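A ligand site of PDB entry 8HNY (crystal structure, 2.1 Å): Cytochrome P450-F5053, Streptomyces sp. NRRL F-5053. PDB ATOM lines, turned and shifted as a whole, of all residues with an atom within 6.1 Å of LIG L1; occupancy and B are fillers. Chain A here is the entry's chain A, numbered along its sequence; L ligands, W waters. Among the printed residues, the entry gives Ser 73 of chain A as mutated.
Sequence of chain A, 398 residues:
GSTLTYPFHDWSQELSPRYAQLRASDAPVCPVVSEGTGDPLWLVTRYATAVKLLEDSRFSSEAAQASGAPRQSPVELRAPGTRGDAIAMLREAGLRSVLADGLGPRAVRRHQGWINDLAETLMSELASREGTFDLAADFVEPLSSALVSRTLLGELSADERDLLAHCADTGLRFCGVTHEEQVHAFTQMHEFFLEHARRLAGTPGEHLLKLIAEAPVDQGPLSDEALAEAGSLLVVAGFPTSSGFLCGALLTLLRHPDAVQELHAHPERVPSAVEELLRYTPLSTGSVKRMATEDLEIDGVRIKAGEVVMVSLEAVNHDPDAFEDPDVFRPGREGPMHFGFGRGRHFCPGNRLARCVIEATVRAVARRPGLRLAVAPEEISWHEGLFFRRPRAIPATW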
ATOM      1  N   GLN A  72     -31.092  31.376 -10.061  1.00  0.00           N
ATOM      2  CA  GLN A  72     -30.604  30.157  -9.434  1.00  0.00           C
ATOM      3  C   GLN A  72     -29.518  30.414  -8.392  1.00  0.00           C
ATOM      4  O   GLN A  72     -29.340  29.575  -7.503  1.00  0.00           O
ATOM      5  CB  GLN A  72     -30.066  29.205 -10.519  1.00  0.00           C
ATOM      6  CG  GLN A  72     -28.685  29.575 -11.026  1.00  0.00           C
ATOM      7  CD  GLN A  72     -28.410  28.977 -12.403  1.00  0.00           C
ATOM      8  OE1 GLN A  72     -28.107  27.793 -12.528  1.00  0.00           O
ATOM      9  NE2 GLN A  72     -28.509  29.795 -13.439  1.00  0.00           N
ATOM     10  N   SER A  73     -28.801  31.544  -8.477  1.00  0.00           N
ATOM     11  CA  SER A  73     -27.703  31.826  -7.549  1.00  0.00           C
ATOM     12  C   SER A  73     -28.217  32.375  -6.220  1.00  0.00           C
ATOM     13  O   SER A  73     -29.176  33.159  -6.198  1.00  0.00           O
ATOM     14  CB  SER A  73     -26.729  32.829  -8.162  1.00  0.00           C
ATOM     15  OG  SER A  73     -25.811  33.314  -7.178  1.00  0.00           O
ATOM     16  N   LEU A  77     -24.892  38.340  -8.700  1.00  0.00           N
ATOM     17  CA  LEU A  77     -23.518  38.143  -9.138  1.00  0.00           C
ATOM     18  C   LEU A  77     -22.882  39.431  -9.644  1.00  0.00           C
ATOM     19  O   LEU A  77     -22.302  39.481 -10.716  1.00  0.00           O
ATOM     20  CB  LEU A  77     -23.467  37.068 -10.214  1.00  0.00           C
ATOM     21  CG  LEU A  77     -24.072  35.721  -9.775  1.00  0.00           C
ATOM     22  CD1 LEU A  77     -23.930  34.646 -10.865  1.00  0.00           C
ATOM     23  CD2 LEU A  77     -23.449  35.275  -8.452  1.00  0.00           C
ATOM     24  N   PHE A 174     -22.788  28.040  -5.597  1.00  0.00           N
ATOM     25  CA  PHE A 174     -24.124  27.760  -5.085  1.00  0.00           C
ATOM     26  C   PHE A 174     -24.145  27.599  -3.570  1.00  0.00           C
ATOM     27  O   PHE A 174     -25.155  27.899  -2.934  1.00  0.00           O
ATOM     28  CB  PHE A 174     -24.683  26.490  -5.721  1.00  0.00           C
ATOM     29  CG  PHE A 174     -25.202  26.687  -7.109  1.00  0.00           C
ATOM     30  CD1 PHE A 174     -26.308  27.475  -7.332  1.00  0.00           C
ATOM     31  CD2 PHE A 174     -24.581  26.075  -8.191  1.00  0.00           C
ATOM     32  CE1 PHE A 174     -26.787  27.649  -8.616  1.00  0.00           C
ATOM     33  CE2 PHE A 174     -25.055  26.247  -9.453  1.00  0.00           C
ATOM     34  CZ  PHE A 174     -26.162  27.037  -9.666  1.00  0.00           C
ATOM     35  N   ALA A 237     -15.622  35.264 -16.519  1.00  0.00           N
ATOM     36  CA  ALA A 237     -15.915  34.518 -17.744  1.00  0.00           C
ATOM     37  C   ALA A 237     -14.769  33.632 -18.209  1.00  0.00           C
ATOM     38  O   ALA A 237     -15.015  32.655 -18.935  1.00  0.00           O
ATOM     39  CB  ALA A 237     -16.272  35.502 -18.876  1.00  0.00           C
ATOM     40  N   THR A 241     -13.663  29.375 -15.547  1.00  0.00           N
ATOM     41  CA  THR A 241     -14.091  28.529 -16.659  1.00  0.00           C
ATOM     42  C   THR A 241     -12.903  27.801 -17.295  1.00  0.00           C
ATOM     43  O   THR A 241     -12.951  26.582 -17.471  1.00  0.00           O
ATOM     44  CB  THR A 241     -14.780  29.399 -17.701  1.00  0.00           C
ATOM     45  OG1 THR A 241     -13.995  30.576 -17.914  1.00  0.00           O
ATOM     46  CG2 THR A 241     -16.140  29.816 -17.203  1.00  0.00           C
ATOM     47  N   LEU A 283     -18.804  21.040 -17.138  1.00  0.00           N
ATOM     48  CA  LEU A 283     -18.173  22.190 -16.510  1.00  0.00           C
ATOM     49  C   LEU A 283     -19.110  22.804 -15.478  1.00  0.00           C
ATOM     50  O   LEU A 283     -18.943  22.604 -14.271  1.00  0.00           O
ATOM     51  CB  LEU A 283     -17.807  23.255 -17.547  1.00  0.00           C
ATOM     52  CG  LEU A 283     -16.928  24.395 -17.036  1.00  0.00           C
ATOM     53  CD1 LEU A 283     -15.566  23.838 -16.677  1.00  0.00           C
ATOM     54  CD2 LEU A 283     -16.798  25.480 -18.101  1.00  0.00           C
ATOM     55  N   SER A 284     -20.114  23.540 -15.952  1.00  0.00           N
ATOM     56  CA  SER A 284     -20.985  24.285 -15.062  1.00  0.00           C
ATOM     57  C   SER A 284     -21.914  23.328 -14.334  1.00  0.00           C
ATOM     58  O   SER A 284     -22.347  22.325 -14.896  1.00  0.00           O
ATOM     59  CB  SER A 284     -21.791  25.325 -15.835  1.00  0.00           C
ATOM     60  OG  SER A 284     -22.798  25.905 -15.016  1.00  0.00           O
ATOM     61  N   THR A 285     -22.184  23.644 -13.055  1.00  0.00           N
ATOM     62  CA  THR A 285     -23.184  22.927 -12.266  1.00  0.00           C
ATOM     63  C   THR A 285     -24.540  23.636 -12.267  1.00  0.00           C
ATOM     64  O   THR A 285     -25.518  23.075 -11.756  1.00  0.00           O
ATOM     65  CB  THR A 285     -22.681  22.731 -10.820  1.00  0.00           C
ATOM     66  OG1 THR A 285     -22.411  23.999 -10.208  1.00  0.00           O
ATOM     67  CG2 THR A 285     -21.400  21.916 -10.838  1.00  0.00           C
ATOM     68  N   GLY A 286     -24.618  24.840 -12.824  1.00  0.00           N
ATOM     69  CA  GLY A 286     -25.895  25.467 -13.023  1.00  0.00           C
ATOM     70  C   GLY A 286     -26.245  25.525 -14.501  1.00  0.00           C
ATOM     71  O   GLY A 286     -25.791  24.687 -15.301  1.00  0.00           O
ATOM     72  N   SER A 287     -27.022  26.524 -14.880  1.00  0.00           N
ATOM     73  CA  SER A 287     -27.599  26.580 -16.215  1.00  0.00           C
ATOM     74  C   SER A 287     -27.381  27.960 -16.805  1.00  0.00           C
ATOM     75  O   SER A 287     -27.293  28.944 -16.070  1.00  0.00           O
ATOM     76  CB  SER A 287     -29.083  26.275 -16.171  1.00  0.00           C
ATOM     77  OG  SER A 287     -29.308  24.886 -15.952  1.00  0.00           O
ATOM     78  N   VAL A 288     -27.249  28.031 -18.142  1.00  0.00           N
ATOM     79  CA  VAL A 288     -27.427  29.334 -18.764  1.00  0.00           C
ATOM     80  C   VAL A 288     -28.868  29.714 -18.492  1.00  0.00           C
ATOM     81  O   VAL A 288     -29.734  28.852 -18.313  1.00  0.00           O
ATOM     82  CB  VAL A 288     -27.131  29.340 -20.265  1.00  0.00           C
ATOM     83  CG1 VAL A 288     -25.767  28.674 -20.609  1.00  0.00           C
ATOM     84  CG2 VAL A 288     -28.271  28.675 -20.974  1.00  0.00           C
ATOM     85  N   LYS A 289     -29.155  31.015 -18.455  1.00  0.00           N
ATOM     86  CA  LYS A 289     -30.523  31.408 -18.109  1.00  0.00           C
ATOM     87  C   LYS A 289     -30.967  32.616 -18.911  1.00  0.00           C
ATOM     88  O   LYS A 289     -30.168  33.493 -19.249  1.00  0.00           O
ATOM     89  CB  LYS A 289     -30.653  31.701 -16.604  1.00  0.00           C
ATOM     90  CG  LYS A 289     -30.163  33.067 -16.233  1.00  0.00           C
ATOM     91  CD  LYS A 289     -28.682  33.051 -15.969  1.00  0.00           C
ATOM     92  CE  LYS A 289     -28.215  34.475 -15.725  1.00  0.00           C
ATOM     93  NZ  LYS A 289     -26.762  34.566 -16.009  1.00  0.00           N
ATOM     94  N   VAL A 311     -31.181  26.538 -19.262  1.00  0.00           N
ATOM     95  CA  VAL A 311     -30.747  25.390 -20.047  1.00  0.00           C
ATOM     96  C   VAL A 311     -29.466  24.836 -19.405  1.00  0.00           C
ATOM     97  O   VAL A 311     -28.497  25.571 -19.214  1.00  0.00           O
ATOM     98  CB  VAL A 311     -30.482  25.740 -21.515  1.00  0.00           C
ATOM     99  CG1 VAL A 311     -30.020  24.502 -22.261  1.00  0.00           C
ATOM    100  CG2 VAL A 311     -31.745  26.268 -22.191  1.00  0.00           C
ATOM    101  N   LEU A 313     -26.395  23.003 -20.114  1.00  0.00           N
ATOM    102  CA  LEU A 313     -25.586  22.555 -21.228  1.00  0.00           C
ATOM    103  C   LEU A 313     -25.113  21.128 -21.003  1.00  0.00           C
ATOM    104  O   LEU A 313     -25.009  20.346 -21.951  1.00  0.00           O
ATOM    105  CB  LEU A 313     -24.411  23.500 -21.443  1.00  0.00           C
ATOM    106  CG  LEU A 313     -24.759  24.991 -21.572  1.00  0.00           C
ATOM    107  CD1 LEU A 313     -23.519  25.859 -21.762  1.00  0.00           C
ATOM    108  CD2 LEU A 313     -25.718  25.185 -22.723  1.00  0.00           C
ATOM    109  N   GLU A 314     -24.867  20.771 -19.746  1.00  0.00           N
ATOM    110  CA  GLU A 314     -24.460  19.404 -19.419  1.00  0.00           C
ATOM    111  C   GLU A 314     -25.523  18.399 -19.843  1.00  0.00           C
ATOM    112  O   GLU A 314     -25.215  17.398 -20.501  1.00  0.00           O
ATOM    113  CB  GLU A 314     -24.171  19.278 -17.922  1.00  0.00           C
ATOM    114  CG  GLU A 314     -22.757  19.727 -17.579  1.00  0.00           C
ATOM    115  CD  GLU A 314     -22.573  21.200 -17.851  1.00  0.00           C
ATOM    116  OE1 GLU A 314     -23.550  21.942 -17.651  1.00  0.00           O
ATOM    117  OE2 GLU A 314     -21.474  21.614 -18.264  1.00  0.00           O
ATOM    118  N   GLY A 340     -21.103  23.077 -25.330  1.00  0.00           N
ATOM    119  CA  GLY A 340     -20.075  23.500 -24.398  1.00  0.00           C
ATOM    120  C   GLY A 340     -19.834  24.983 -24.340  1.00  0.00           C
ATOM    121  O   GLY A 340     -19.402  25.513 -23.312  1.00  0.00           O
ATOM    122  N   PHE A 387     -19.806  26.960  -9.070  1.00  0.00           N
ATOM    123  CA  PHE A 387     -20.508  26.992 -10.363  1.00  0.00           C
ATOM    124  C   PHE A 387     -19.765  26.171 -11.399  1.00  0.00           C
ATOM    125  O   PHE A 387     -20.358  25.408 -12.184  1.00  0.00           O
ATOM    126  CB  PHE A 387     -20.642  28.438 -10.866  1.00  0.00           C
ATOM    127  CG  PHE A 387     -21.625  29.300 -10.089  1.00  0.00           C
ATOM    128  CD1 PHE A 387     -22.439  28.755  -9.096  1.00  0.00           C
ATOM    129  CD2 PHE A 387     -21.713  30.676 -10.356  1.00  0.00           C
ATOM    130  CE1 PHE A 387     -23.337  29.571  -8.377  1.00  0.00           C
ATOM    131  CE2 PHE A 387     -22.613  31.494  -9.627  1.00  0.00           C
ATOM    132  CZ  PHE A 387     -23.423  30.934  -8.641  1.00  0.00           C
ATOM    133  N   PHE A 388     -18.449  26.313 -11.439  1.00  0.00           N
ATOM    134  CA  PHE A 388     -17.615  25.684 -12.447  1.00  0.00           C
ATOM    135  C   PHE A 388     -16.776  24.607 -11.785  1.00  0.00           C
ATOM    136  O   PHE A 388     -15.915  24.921 -10.940  1.00  0.00           O
ATOM    137  CB  PHE A 388     -16.793  26.747 -13.160  1.00  0.00           C
ATOM    138  CG  PHE A 388     -17.656  27.842 -13.746  1.00  0.00           C
ATOM    139  CD1 PHE A 388     -18.384  27.609 -14.910  1.00  0.00           C
ATOM    140  CD2 PHE A 388     -17.786  29.074 -13.102  1.00  0.00           C
ATOM    141  CE1 PHE A 388     -19.197  28.579 -15.436  1.00  0.00           C
ATOM    142  CE2 PHE A 388     -18.605  30.070 -13.633  1.00  0.00           C
ATOM    143  CZ  PHE A 388     -19.311  29.822 -14.821  1.00  0.00           C
HETATM  144  C1  LIG L   1     -23.551  30.210 -16.145  1.00  0.00           C
HETATM  145  C2  LIG L   1     -23.997  29.926 -17.586  1.00  0.00           C
HETATM  146  C3  LIG L   1     -23.097  28.748 -18.020  1.00  0.00           C
HETATM  147  C4  LIG L   1     -23.475  27.402 -18.104  1.00  0.00           C
HETATM  148  C5  LIG L   1     -24.599  31.111 -15.478  1.00  0.00           C
HETATM  149  C6  LIG L   1     -23.761  30.302 -13.304  1.00  0.00           C
HETATM  150  C7  LIG L   1     -24.887  30.161 -12.074  1.00  0.00           C
HETATM  151  C8  LIG L   1     -25.770  31.429 -12.167  1.00  0.00           C
HETATM  152  C9  LIG L   1     -25.640  31.958 -13.452  1.00  0.00           C
HETATM  153  C10 LIG L   1     -23.378  28.920 -13.845  1.00  0.00           C
HETATM  154  C11 LIG L   1     -21.296  27.548 -18.608  1.00  0.00           C
HETATM  155  C12 LIG L   1     -19.929  27.287 -18.955  1.00  0.00           C
HETATM  156  C13 LIG L   1     -19.012  28.334 -19.029  1.00  0.00           C
HETATM  157  C14 LIG L   1     -19.436  29.650 -18.743  1.00  0.00           C
HETATM  158  C15 LIG L   1     -20.768  29.902 -18.367  1.00  0.00           C
HETATM  159  C16 LIG L   1     -21.707  28.832 -18.314  1.00  0.00           C
HETATM  160  F1  LIG L   1     -21.171  31.179 -18.112  1.00  0.00           F
HETATM  161  N1  LIG L   1     -24.456  30.980 -14.122  1.00  0.00           N
HETATM  162  N2  LIG L   1     -23.263  28.874 -15.424  1.00  0.00           N
HETATM  163  N3  LIG L   1     -22.381  26.709 -18.466  1.00  0.00           N
HETATM  164  O1  LIG L   1     -25.356  31.813 -16.075  1.00  0.00           O
HETATM  165  O2  LIG L   1     -23.162  27.966 -13.127  1.00  0.00           O
HETATM  166  C1  LG2 L   2     -20.242  33.184 -22.427  1.00  0.00           C
HETATM  167  C2  LG2 L   2     -15.823  35.114 -22.304  1.00  0.00           C
HETATM  168  C3  LG2 L   2     -13.929  30.725 -21.697  1.00  0.00           C
HETATM  169  C4  LG2 L   2     -18.337  28.805 -22.046  1.00  0.00           C
HETATM  170  C5  LG2 L   2     -19.204  34.073 -22.381  1.00  0.00           C
HETATM  171  C6  LG2 L   2     -19.352  35.511 -22.350  1.00  0.00           C
HETATM  172  C7  LG2 L   2     -18.145  36.048 -22.319  1.00  0.00           C
HETATM  173  C8  LG2 L   2     -17.178  34.961 -22.322  1.00  0.00           C
HETATM  174  C9  LG2 L   2     -17.819  37.558 -22.281  1.00  0.00           C
HETATM  175  C10 LG2 L   2     -20.684  36.275 -22.355  1.00  0.00           C
HETATM  176  C11 LG2 L   2     -21.323  36.228 -23.747  1.00  0.00           C
HETATM  177  C12 LG2 L   2     -22.699  36.844 -23.675  1.00  0.00           C
HETATM  178  O1  LG2 L   2     -23.058  37.573 -24.612  1.00  0.00           O
HETATM  179  O2  LG2 L   2     -23.412  36.640 -22.655  1.00  0.00           O
HETATM  180  C13 LG2 L   2     -14.928  34.089 -22.176  1.00  0.00           C
HETATM  181  C14 LG2 L   2     -13.499  34.233 -22.091  1.00  0.00           C
HETATM  182  C15 LG2 L   2     -12.994  33.012 -21.903  1.00  0.00           C
HETATM  183  C16 LG2 L   2     -14.077  32.072 -21.867  1.00  0.00           C
HETATM  184  C17 LG2 L   2     -12.763  35.588 -22.208  1.00  0.00           C
HETATM  185  C18 LG2 L   2     -11.524  32.578 -21.811  1.00  0.00           C
HETATM  186  C19 LG2 L   2     -10.553  33.336 -22.324  1.00  0.00           C
HETATM  187  C20 LG2 L   2     -14.949  29.827 -21.697  1.00  0.00           C
HETATM  188  C21 LG2 L   2     -14.829  28.403 -21.519  1.00  0.00           C
HETATM  189  C22 LG2 L   2     -16.036  27.875 -21.614  1.00  0.00           C
HETATM  190  C23 LG2 L   2     -16.978  28.948 -21.892  1.00  0.00           C
HETATM  191  C24 LG2 L   2     -13.510  27.608 -21.244  1.00  0.00           C
HETATM  192  C25 LG2 L   2     -16.353  26.377 -21.487  1.00  0.00           C
HETATM  193  C26 LG2 L   2     -17.594  25.942 -21.263  1.00  0.00           C
HETATM  194  C27 LG2 L   2     -19.250  29.806 -22.164  1.00  0.00           C
HETATM  195  C28 LG2 L   2     -20.682  29.661 -22.321  1.00  0.00           C
HETATM  196  C29 LG2 L   2     -21.205  30.873 -22.428  1.00  0.00           C
HETATM  197  C30 LG2 L   2     -20.119  31.827 -22.363  1.00  0.00           C
HETATM  198  C31 LG2 L   2     -21.519  28.367 -22.357  1.00  0.00           C
HETATM  199  C32 LG2 L   2     -22.702  31.178 -22.629  1.00  0.00           C
HETATM  200  C33 LG2 L   2     -23.408  31.647 -21.364  1.00  0.00           C
HETATM  201  C34 LG2 L   2     -24.817  32.043 -21.748  1.00  0.00           C
HETATM  202  O3  LG2 L   2     -25.222  31.777 -22.916  1.00  0.00           O
HETATM  203  O4  LG2 L   2     -25.527  32.610 -20.881  1.00  0.00           O
HETATM  204  N1  LG2 L   2     -17.867  33.760 -22.365  1.00  0.00           N
HETATM  205  N2  LG2 L   2     -15.257  32.767 -22.038  1.00  0.00           N
HETATM  206  N3  LG2 L   2     -16.270  30.122 -21.934  1.00  0.00           N
HETATM  207  N4  LG2 L   2     -18.918  31.141 -22.200  1.00  0.00           N
HETATM  208 FE1  LG2 L   2     -17.094  31.897 -22.158  1.00  0.00          FE
HETATM  209  O   HOH W   1     -21.048  24.086 -18.587  1.00  0.00           O
HETATM  210  O   HOH W   2     -25.136  24.503 -17.898  1.00  0.00           O
HETATM  211  O   HOH W   3     -26.866  32.749 -18.686  1.00  0.00           O
HETATM  212  O   HOH W   4     -28.107  33.579 -11.213  1.00  0.00           O
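Water W1 lies within hydrogen-bond range of the side-chain carboxylate of Glu 314 (2.5 Å), the backbone NH of Ser 284 (2.8 Å) and a nitrogen (N3) of LIG L1 (2.9 Å). Water W3 lies within hydrogen-bond range of O4 of LG2 L2 (2.6 Å), N of Lys 289 (2.9 Å) and O1 of LIG L1 (3.2 Å). Water W2 lies within hydrogen-bond range of O of Gly 286 (2.7 Å), N of Leu 313 (3.0 Å) and OE1 of Glu 314 (3.0 Å).
The backbone carbonyl oxygen (O) of Ser 287 sits close to an oxygen (O1) of LIG L1, 3.5 Å away. Residues that only touch LIG L1: Gln 72 (3.4 Å), Leu 77 (3.9 Å), Thr 241 (3.6 Å), Leu 283 (3.7 Å), Val 288 (3.6 Å), Leu 313 (3.6 Å), Phe 387 (3.4 Å) and Phe 388 (3.5 Å). The nearest printed residue that does not touch LIG L1 is Phe 174 (4.1 Å).
OG of Ser 284 is in hydrogen-bond range of O2 of LIG L1, at 2.8 Å. The side-chain amino group of Lys 289 lies within hydrogen-bond range of an oxygen (O1) of LIG L1 (3.1 Å). O2 of LIG L1 sits at hydrogen-bond distance from N of Gly 286 (3.5 Å).
OG of Ser 284 is in hydrogen-bond range of N of Gly 286, 3.0 Å away. The side-chain carboxylate (OE2) of Glu 314 sits at hydrogen-bond distance from the backbone NH (N) of Ser 284 (3.3 Å). The backbone carbonyl oxygen (O) of Phe 387 sits at hydrogen-bond distance from the backbone NH (N) of Thr 285. OE1 of Gln 72 sits at hydrogen-bond distance from N of Ser 287 (2.9 Å). The backbone carbonyl oxygen (O) of Val 311 sits close to the side-chain hydroxyl (OG) of Ser 287 (3.4 Å). The backbone carbonyl oxygen (O) of Val 288 is in hydrogen-bond range of the backbone NH (N) of Val 311 (2.9 Å). The side-chain hydroxyl (OG1) of Thr 241 is in hydrogen-bond range of the backbone carbonyl oxygen (O) of Ala 237, at 2.5 Å. N of Leu 283 is in hydrogen-bond range of OE2 of Glu 314 (3.0 Å).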
